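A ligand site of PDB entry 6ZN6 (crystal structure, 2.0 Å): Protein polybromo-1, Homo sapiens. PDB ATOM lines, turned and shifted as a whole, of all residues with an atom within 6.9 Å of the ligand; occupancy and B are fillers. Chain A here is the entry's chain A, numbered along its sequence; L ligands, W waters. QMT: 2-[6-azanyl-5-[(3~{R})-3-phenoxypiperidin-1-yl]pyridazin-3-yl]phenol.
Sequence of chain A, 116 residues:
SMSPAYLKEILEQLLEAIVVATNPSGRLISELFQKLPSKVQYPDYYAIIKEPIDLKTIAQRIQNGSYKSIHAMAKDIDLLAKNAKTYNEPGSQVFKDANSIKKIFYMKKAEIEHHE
Merely in contact with the ligand: Ile 53 (3.3 Å), Tyr 42 (3.4 Å), Leu 32 (3.5 Å), Ala 84 (3.5 Å), Phe 33 (3.6 Å), Val 94 (3.7 Å), Tyr 87 (3.8 Å), Pro 37 (3.8 Å), Lys 35 (3.8 Å), Asp 54 (3.9 Å) and Leu 36 (3.96 Å). 13 residues have an atom within 4 Å of the ligand: Leu 32, Phe 33, Lys 35, Leu 36, Pro 37, Tyr 42, Tyr 45, Ile 53, Asp 54, Ala 84, Tyr 87, Asn 88 and Val 94.
The side-chain hydroxyl (OH) of Tyr 45 sits at hydrogen-bond distance from an oxygen (O1) of the ligand (2.8 Å). The side-chain amide nitrogen (ND2) of Asn 88 is in hydrogen-bond range of a nitrogen (N3) of the ligand, at 3.0 Å.
Water W1 lies within hydrogen-bond range of the side-chain hydroxyl (OH) of Tyr 45 (2.6 Å), the backbone carbonyl oxygen (O) of Ile 53 (2.6 Å) and the side-chain amide nitrogen (ND2) of Asn 83 (3.1 Å).
The side-chain amide nitrogen (ND2) of Asn 88 lies within hydrogen-bond range of the backbone carbonyl oxygen (O) of Ala 84 (2.8 Å). The backbone carbonyl oxygen of Phe 33 lies within hydrogen-bond range of the backbone NH of Leu 55 (2.8 Å). OD2 of Asp 54 sits at hydrogen-bond distance from N of Leu 36 (2.7 Å).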
ATOM      1  N   GLU A  31     -15.257 -22.307  24.448  1.00  0.00           N
ATOM      2  CA  GLU A  31     -15.431 -22.792  25.819  1.00  0.00           C
ATOM      3  C   GLU A  31     -14.522 -23.970  26.145  1.00  0.00           C
ATOM      4  O   GLU A  31     -13.889 -24.017  27.219  1.00  0.00           O
ATOM      5  CB  GLU A  31     -16.880 -23.160  26.070  1.00  0.00           C
ATOM      6  CG  GLU A  31     -17.249 -22.920  27.497  1.00  0.00           C
ATOM      7  CD  GLU A  31     -16.988 -21.478  27.927  1.00  0.00           C
ATOM      8  OE1 GLU A  31     -16.047 -21.271  28.727  1.00  0.00           O
ATOM      9  OE2 GLU A  31     -17.712 -20.567  27.470  1.00  0.00           O
ATOM     10  N   LEU A  32     -14.448 -24.962  25.252  1.00  0.00           N
ATOM     11  CA  LEU A  32     -13.647 -26.140  25.564  1.00  0.00           C
ATOM     12  C   LEU A  32     -12.188 -25.765  25.789  1.00  0.00           C
ATOM     13  O   LEU A  32     -11.491 -26.420  26.565  1.00  0.00           O
ATOM     14  CB  LEU A  32     -13.769 -27.168  24.427  1.00  0.00           C
ATOM     15  CG  LEU A  32     -12.839 -28.382  24.600  1.00  0.00           C
ATOM     16  CD1 LEU A  32     -13.603 -29.684  24.472  1.00  0.00           C
ATOM     17  CD2 LEU A  32     -11.644 -28.328  23.627  1.00  0.00           C
ATOM     18  N   PHE A  33     -11.728 -24.716  25.134  1.00  0.00           N
ATOM     19  CA  PHE A  33     -10.321 -24.335  25.204  1.00  0.00           C
ATOM     20  C   PHE A  33      -9.992 -23.409  26.383  1.00  0.00           C
ATOM     21  O   PHE A  33      -8.823 -22.991  26.517  1.00  0.00           O
ATOM     22  CB  PHE A  33      -9.922 -23.700  23.870  1.00  0.00           C
ATOM     23  CG  PHE A  33     -10.094 -24.627  22.695  1.00  0.00           C
ATOM     24  CD1 PHE A  33      -9.292 -25.756  22.570  1.00  0.00           C
ATOM     25  CD2 PHE A  33     -11.075 -24.390  21.738  1.00  0.00           C
ATOM     26  CE1 PHE A  33      -9.445 -26.622  21.484  1.00  0.00           C
ATOM     27  CE2 PHE A  33     -11.233 -25.243  20.656  1.00  0.00           C
ATOM     28  CZ  PHE A  33     -10.423 -26.366  20.521  1.00  0.00           C
ATOM     29  N   GLN A  34     -10.966 -23.090  27.234  1.00  0.00           N
ATOM     30  CA  GLN A  34     -10.699 -22.187  28.351  1.00  0.00           C
ATOM     31  C   GLN A  34      -9.690 -22.791  29.312  1.00  0.00           C
ATOM     32  O   GLN A  34      -8.689 -22.149  29.673  1.00  0.00           O
ATOM     33  CB  GLN A  34     -11.991 -21.830  29.083  1.00  0.00           C
ATOM     34  CG  GLN A  34     -12.883 -20.818  28.356  1.00  0.00           C
ATOM     35  CD  GLN A  34     -12.280 -19.418  28.236  1.00  0.00           C
ATOM     36  OE1 GLN A  34     -11.194 -19.117  28.761  1.00  0.00           O
ATOM     37  NE2 GLN A  34     -12.987 -18.552  27.539  1.00  0.00           N
ATOM     38  N   LYS A  35      -9.927 -24.036  29.749  1.00  0.00           N
ATOM     39  CA  LYS A  35      -9.159 -24.641  30.818  1.00  0.00           C
ATOM     40  C   LYS A  35      -8.694 -26.015  30.373  1.00  0.00           C
ATOM     41  O   LYS A  35      -9.491 -26.798  29.852  1.00  0.00           O
ATOM     42  CB  LYS A  35      -9.984 -24.744  32.110  1.00  0.00           C
ATOM     43  N   LEU A  36      -7.393 -26.274  30.528  1.00  0.00           N
ATOM     44  CA  LEU A  36      -6.781 -27.537  30.155  1.00  0.00           C
ATOM     45  C   LEU A  36      -7.547 -28.705  30.768  1.00  0.00           C
ATOM     46  O   LEU A  36      -8.156 -28.543  31.842  1.00  0.00           O
ATOM     47  CB  LEU A  36      -5.328 -27.587  30.632  1.00  0.00           C
ATOM     48  CG  LEU A  36      -4.277 -26.823  29.846  1.00  0.00           C
ATOM     49  CD1 LEU A  36      -3.088 -26.503  30.769  1.00  0.00           C
ATOM     50  CD2 LEU A  36      -3.844 -27.634  28.648  1.00  0.00           C
ATOM     51  N   PRO A  37      -7.560 -29.863  30.126  1.00  0.00           N
ATOM     52  CA  PRO A  37      -8.211 -31.025  30.744  1.00  0.00           C
ATOM     53  C   PRO A  37      -7.435 -31.502  31.963  1.00  0.00           C
ATOM     54  O   PRO A  37      -6.201 -31.445  32.013  1.00  0.00           O
ATOM     55  CB  PRO A  37      -8.214 -32.074  29.628  1.00  0.00           C
ATOM     56  CG  PRO A  37      -7.102 -31.684  28.719  1.00  0.00           C
ATOM     57  CD  PRO A  37      -6.939 -30.193  28.824  1.00  0.00           C
ATOM     58  N   TYR A  42      -7.365 -37.145  32.370  1.00  0.00           N
ATOM     59  CA  TYR A  42      -6.803 -37.212  31.027  1.00  0.00           C
ATOM     60  C   TYR A  42      -5.273 -37.222  31.043  1.00  0.00           C
ATOM     61  O   TYR A  42      -4.621 -36.337  30.490  1.00  0.00           O
ATOM     62  CB  TYR A  42      -7.330 -36.052  30.178  1.00  0.00           C
ATOM     63  CG  TYR A  42      -8.829 -36.139  29.991  1.00  0.00           C
ATOM     64  CD1 TYR A  42      -9.366 -36.952  29.012  1.00  0.00           C
ATOM     65  CD2 TYR A  42      -9.701 -35.444  30.825  1.00  0.00           C
ATOM     66  CE1 TYR A  42     -10.739 -37.064  28.840  1.00  0.00           C
ATOM     67  CE2 TYR A  42     -11.075 -35.561  30.670  1.00  0.00           C
ATOM     68  CZ  TYR A  42     -11.582 -36.364  29.670  1.00  0.00           C
ATOM     69  OH  TYR A  42     -12.940 -36.469  29.494  1.00  0.00           O
ATOM     70  N   TYR A  45      -3.521 -36.905  27.543  1.00  0.00           N
ATOM     71  CA  TYR A  45      -3.271 -35.571  26.999  1.00  0.00           C
ATOM     72  C   TYR A  45      -1.861 -35.105  27.339  1.00  0.00           C
ATOM     73  O   TYR A  45      -1.121 -34.624  26.469  1.00  0.00           O
ATOM     74  CB  TYR A  45      -4.301 -34.564  27.527  1.00  0.00           C
ATOM     75  CG  TYR A  45      -4.213 -33.197  26.826  1.00  0.00           C
ATOM     76  CD1 TYR A  45      -3.303 -32.227  27.260  1.00  0.00           C
ATOM     77  CD2 TYR A  45      -5.022 -32.899  25.723  1.00  0.00           C
ATOM     78  CE1 TYR A  45      -3.211 -30.973  26.604  1.00  0.00           C
ATOM     79  CE2 TYR A  45      -4.932 -31.654  25.071  1.00  0.00           C
ATOM     80  CZ  TYR A  45      -4.023 -30.693  25.508  1.00  0.00           C
ATOM     81  OH  TYR A  45      -3.934 -29.457  24.860  1.00  0.00           O
ATOM     82  N   ILE A  49       1.107 -34.028  24.864  1.00  0.00           N
ATOM     83  CA  ILE A  49       1.272 -32.589  24.672  1.00  0.00           C
ATOM     84  C   ILE A  49       2.402 -32.093  25.583  1.00  0.00           C
ATOM     85  O   ILE A  49       2.237 -31.998  26.806  1.00  0.00           O
ATOM     86  CB  ILE A  49      -0.043 -31.828  24.960  1.00  0.00           C
ATOM     87  CG1 ILE A  49      -1.138 -32.268  23.981  1.00  0.00           C
ATOM     88  CG2 ILE A  49       0.170 -30.313  24.880  1.00  0.00           C
ATOM     89  CD1 ILE A  49      -0.692 -32.327  22.524  1.00  0.00           C
ATOM     90  N   PRO A  52       1.431 -27.821  27.337  1.00  0.00           N
ATOM     91  CA  PRO A  52       0.007 -27.513  27.481  1.00  0.00           C
ATOM     92  C   PRO A  52      -0.217 -26.032  27.662  1.00  0.00           C
ATOM     93  O   PRO A  52       0.523 -25.360  28.390  1.00  0.00           O
ATOM     94  CB  PRO A  52      -0.394 -28.288  28.750  1.00  0.00           C
ATOM     95  CG  PRO A  52       0.595 -29.392  28.836  1.00  0.00           C
ATOM     96  CD  PRO A  52       1.885 -28.782  28.355  1.00  0.00           C
ATOM     97  N   ILE A  53      -1.255 -25.508  27.008  1.00  0.00           N
ATOM     98  CA  ILE A  53      -1.658 -24.117  27.194  1.00  0.00           C
ATOM     99  C   ILE A  53      -3.163 -24.056  26.942  1.00  0.00           C
ATOM    100  O   ILE A  53      -3.719 -24.888  26.233  1.00  0.00           O
ATOM    101  CB  ILE A  53      -0.864 -23.156  26.283  1.00  0.00           C
ATOM    102  CG1 ILE A  53      -1.052 -21.699  26.717  1.00  0.00           C
ATOM    103  CG2 ILE A  53      -1.230 -23.364  24.754  1.00  0.00           C
ATOM    104  CD1 ILE A  53      -0.164 -20.704  25.968  1.00  0.00           C
ATOM    105  N   ASP A  54      -3.827 -23.061  27.561  1.00  0.00           N
ATOM    106  CA  ASP A  54      -5.270 -22.885  27.384  1.00  0.00           C
ATOM    107  C   ASP A  54      -5.589 -21.392  27.350  1.00  0.00           C
ATOM    108  O   ASP A  54      -4.716 -20.549  27.591  1.00  0.00           O
ATOM    109  CB  ASP A  54      -6.079 -23.601  28.497  1.00  0.00           C
ATOM    110  CG  ASP A  54      -5.637 -23.211  29.906  1.00  0.00           C
ATOM    111  OD1 ASP A  54      -5.000 -22.130  30.081  1.00  0.00           O
ATOM    112  OD2 ASP A  54      -5.922 -23.992  30.846  1.00  0.00           O
ATOM    113  N   LEU A  55      -6.845 -21.061  27.055  1.00  0.00           N
ATOM    114  CA  LEU A  55      -7.178 -19.647  26.884  1.00  0.00           C
ATOM    115  C   LEU A  55      -7.113 -18.871  28.194  1.00  0.00           C
ATOM    116  O   LEU A  55      -6.825 -17.665  28.179  1.00  0.00           O
ATOM    117  CB  LEU A  55      -8.557 -19.475  26.240  1.00  0.00           C
ATOM    118  CG  LEU A  55      -8.716 -19.971  24.803  1.00  0.00           C
ATOM    119  CD1 LEU A  55     -10.188 -19.957  24.400  1.00  0.00           C
ATOM    120  CD2 LEU A  55      -7.863 -19.126  23.831  1.00  0.00           C
ATOM    121  N   LEU A  80      -1.622 -23.511  21.063  1.00  0.00           N
ATOM    122  CA  LEU A  80      -2.869 -24.078  21.563  1.00  0.00           C
ATOM    123  C   LEU A  80      -3.577 -24.874  20.470  1.00  0.00           C
ATOM    124  O   LEU A  80      -3.996 -26.021  20.684  1.00  0.00           O
ATOM    125  CB  LEU A  80      -3.775 -22.969  22.100  1.00  0.00           C
ATOM    126  CG  LEU A  80      -5.063 -23.364  22.828  1.00  0.00           C
ATOM    127  CD1 LEU A  80      -5.393 -22.339  23.885  1.00  0.00           C
ATOM    128  CD2 LEU A  80      -6.238 -23.500  21.886  1.00  0.00           C
ATOM    129  N   ALA A  81      -3.671 -24.290  19.264  1.00  0.00           N
ATOM    130  CA  ALA A  81      -4.362 -24.979  18.178  1.00  0.00           C
ATOM    131  C   ALA A  81      -3.604 -26.222  17.713  1.00  0.00           C
ATOM    132  O   ALA A  81      -4.227 -27.240  17.388  1.00  0.00           O
ATOM    133  CB  ALA A  81      -4.588 -24.010  17.007  1.00  0.00           C
ATOM    134  N   ASN A  83      -1.591 -28.102  19.582  1.00  0.00           N
ATOM    135  CA  ASN A  83      -1.839 -29.072  20.638  1.00  0.00           C
ATOM    136  C   ASN A  83      -3.186 -29.746  20.433  1.00  0.00           C
ATOM    137  O   ASN A  83      -3.286 -30.978  20.391  1.00  0.00           O
ATOM    138  CB  ASN A  83      -1.773 -28.382  22.007  1.00  0.00           C
ATOM    139  CG  ASN A  83      -0.344 -28.077  22.446  1.00  0.00           C
ATOM    140  OD1 ASN A  83       0.627 -28.580  21.862  1.00  0.00           O
ATOM    141  ND2 ASN A  83      -0.201 -27.272  23.508  1.00  0.00           N
ATOM    142  N   ALA A  84      -4.246 -28.953  20.287  1.00  0.00           N
ATOM    143  CA  ALA A  84      -5.568 -29.509  20.031  1.00  0.00           C
ATOM    144  C   ALA A  84      -5.585 -30.405  18.797  1.00  0.00           C
ATOM    145  O   ALA A  84      -6.197 -31.478  18.805  1.00  0.00           O
ATOM    146  CB  ALA A  84      -6.592 -28.397  19.863  1.00  0.00           C
ATOM    147  N   LYS A  85      -4.901 -29.987  17.728  1.00  0.00           N
ATOM    148  CA  LYS A  85      -4.916 -30.728  16.478  1.00  0.00           C
ATOM    149  C   LYS A  85      -3.998 -31.957  16.514  1.00  0.00           C
ATOM    150  O   LYS A  85      -4.033 -32.772  15.590  1.00  0.00           O
ATOM    151  CB  LYS A  85      -4.547 -29.800  15.323  1.00  0.00           C
ATOM    152  CG  LYS A  85      -5.648 -28.759  15.042  1.00  0.00           C
ATOM    153  CD  LYS A  85      -5.141 -27.574  14.217  1.00  0.00           C
ATOM    154  CE  LYS A  85      -4.654 -28.026  12.847  1.00  0.00           C
ATOM    155  NZ  LYS A  85      -4.098 -26.896  12.007  1.00  0.00           N
ATOM    156  N   TYR A  87      -3.794 -33.920  19.678  1.00  0.00           N
ATOM    157  CA  TYR A  87      -4.484 -34.859  20.544  1.00  0.00           C
ATOM    158  C   TYR A  87      -5.789 -35.355  19.922  1.00  0.00           C
ATOM    159  O   TYR A  87      -6.252 -36.433  20.281  1.00  0.00           O
ATOM    160  CB  TYR A  87      -4.746 -34.201  21.895  1.00  0.00           C
ATOM    161  CG  TYR A  87      -5.398 -35.099  22.924  1.00  0.00           C
ATOM    162  CD1 TYR A  87      -4.674 -36.120  23.554  1.00  0.00           C
ATOM    163  CD2 TYR A  87      -6.733 -34.927  23.266  1.00  0.00           C
ATOM    164  CE1 TYR A  87      -5.264 -36.930  24.497  1.00  0.00           C
ATOM    165  CE2 TYR A  87      -7.329 -35.729  24.199  1.00  0.00           C
ATOM    166  CZ  TYR A  87      -6.596 -36.735  24.815  1.00  0.00           C
ATOM    167  OH  TYR A  87      -7.201 -37.547  25.744  1.00  0.00           O
ATOM    168  N   ASN A  88      -6.380 -34.595  19.005  1.00  0.00           N
ATOM    169  CA  ASN A  88      -7.652 -34.931  18.394  1.00  0.00           C
ATOM    170  C   ASN A  88      -7.458 -35.136  16.899  1.00  0.00           C
ATOM    171  O   ASN A  88      -6.555 -34.558  16.284  1.00  0.00           O
ATOM    172  CB  ASN A  88      -8.700 -33.830  18.666  1.00  0.00           C
ATOM    173  CG  ASN A  88      -8.839 -33.507  20.153  1.00  0.00           C
ATOM    174  OD1 ASN A  88      -9.640 -34.128  20.873  1.00  0.00           O
ATOM    175  ND2 ASN A  88      -8.052 -32.548  20.622  1.00  0.00           N
ATOM    176  N   VAL A  94     -13.169 -30.945  18.048  1.00  0.00           N
ATOM    177  CA  VAL A  94     -12.110 -30.146  18.695  1.00  0.00           C
ATOM    178  C   VAL A  94     -11.111 -29.639  17.648  1.00  0.00           C
ATOM    179  O   VAL A  94     -10.698 -28.468  17.681  1.00  0.00           O
ATOM    180  CB  VAL A  94     -11.396 -30.960  19.786  1.00  0.00           C
ATOM    181  CG1 VAL A  94     -10.344 -30.067  20.454  1.00  0.00           C
ATOM    182  CG2 VAL A  94     -12.387 -31.502  20.830  1.00  0.00           C
HETATM  183  C1  QMT L   1     -10.088 -31.708  25.453  1.00  0.00           C
HETATM  184  N2  QMT L   1      -8.206 -30.571  23.775  1.00  0.00           N
HETATM  185  C3  QMT L   1     -13.304 -32.352  27.047  1.00  0.00           C
HETATM  186  C4  QMT L   1     -13.207 -33.831  27.422  1.00  0.00           C
HETATM  187  C5  QMT L   1     -12.126 -34.527  26.611  1.00  0.00           C
HETATM  188  C6  QMT L   1     -13.309 -35.428  24.658  1.00  0.00           C
HETATM  189  C7  QMT L   1     -13.578 -36.621  25.290  1.00  0.00           C
HETATM  190  N   QMT L   1     -10.357 -33.386  23.718  1.00  0.00           N
HETATM  191  C   QMT L   1      -9.735 -32.297  24.214  1.00  0.00           C
HETATM  192  O   QMT L   1     -12.464 -34.478  25.186  1.00  0.00           O
HETATM  193  C10 QMT L   1     -14.745 -36.046  22.851  1.00  0.00           C
HETATM  194  C11 QMT L   1     -13.891 -35.131  23.435  1.00  0.00           C
HETATM  195  C12 QMT L   1     -10.803 -33.811  26.744  1.00  0.00           C
HETATM  196  C13 QMT L   1      -9.472 -30.510  25.799  1.00  0.00           C
HETATM  197  C14 QMT L   1      -8.529 -29.968  24.917  1.00  0.00           C
HETATM  198  C15 QMT L   1      -7.862 -28.656  25.183  1.00  0.00           C
HETATM  199  C16 QMT L   1      -6.756 -28.233  24.427  1.00  0.00           C
HETATM  200  C17 QMT L   1      -6.158 -27.000  24.681  1.00  0.00           C
HETATM  201  C18 QMT L   1      -6.657 -26.176  25.676  1.00  0.00           C
HETATM  202  C19 QMT L   1      -7.739 -26.581  26.431  1.00  0.00           C
HETATM  203  C2  QMT L   1     -11.952 -31.676  27.109  1.00  0.00           C
HETATM  204  C20 QMT L   1      -8.329 -27.812  26.185  1.00  0.00           C
HETATM  205  C8  QMT L   1     -14.438 -37.527  24.695  1.00  0.00           C
HETATM  206  C9  QMT L   1     -15.021 -37.240  23.476  1.00  0.00           C
HETATM  207  N1  QMT L   1     -10.957 -32.419  26.343  1.00  0.00           N
HETATM  208  N3  QMT L   1      -8.801 -31.735  23.415  1.00  0.00           N
HETATM  209  O1  QMT L   1      -6.257 -29.012  23.439  1.00  0.00           O
HETATM  210  O   HOH W   1      -2.875 -27.104  25.115  1.00  0.00           O
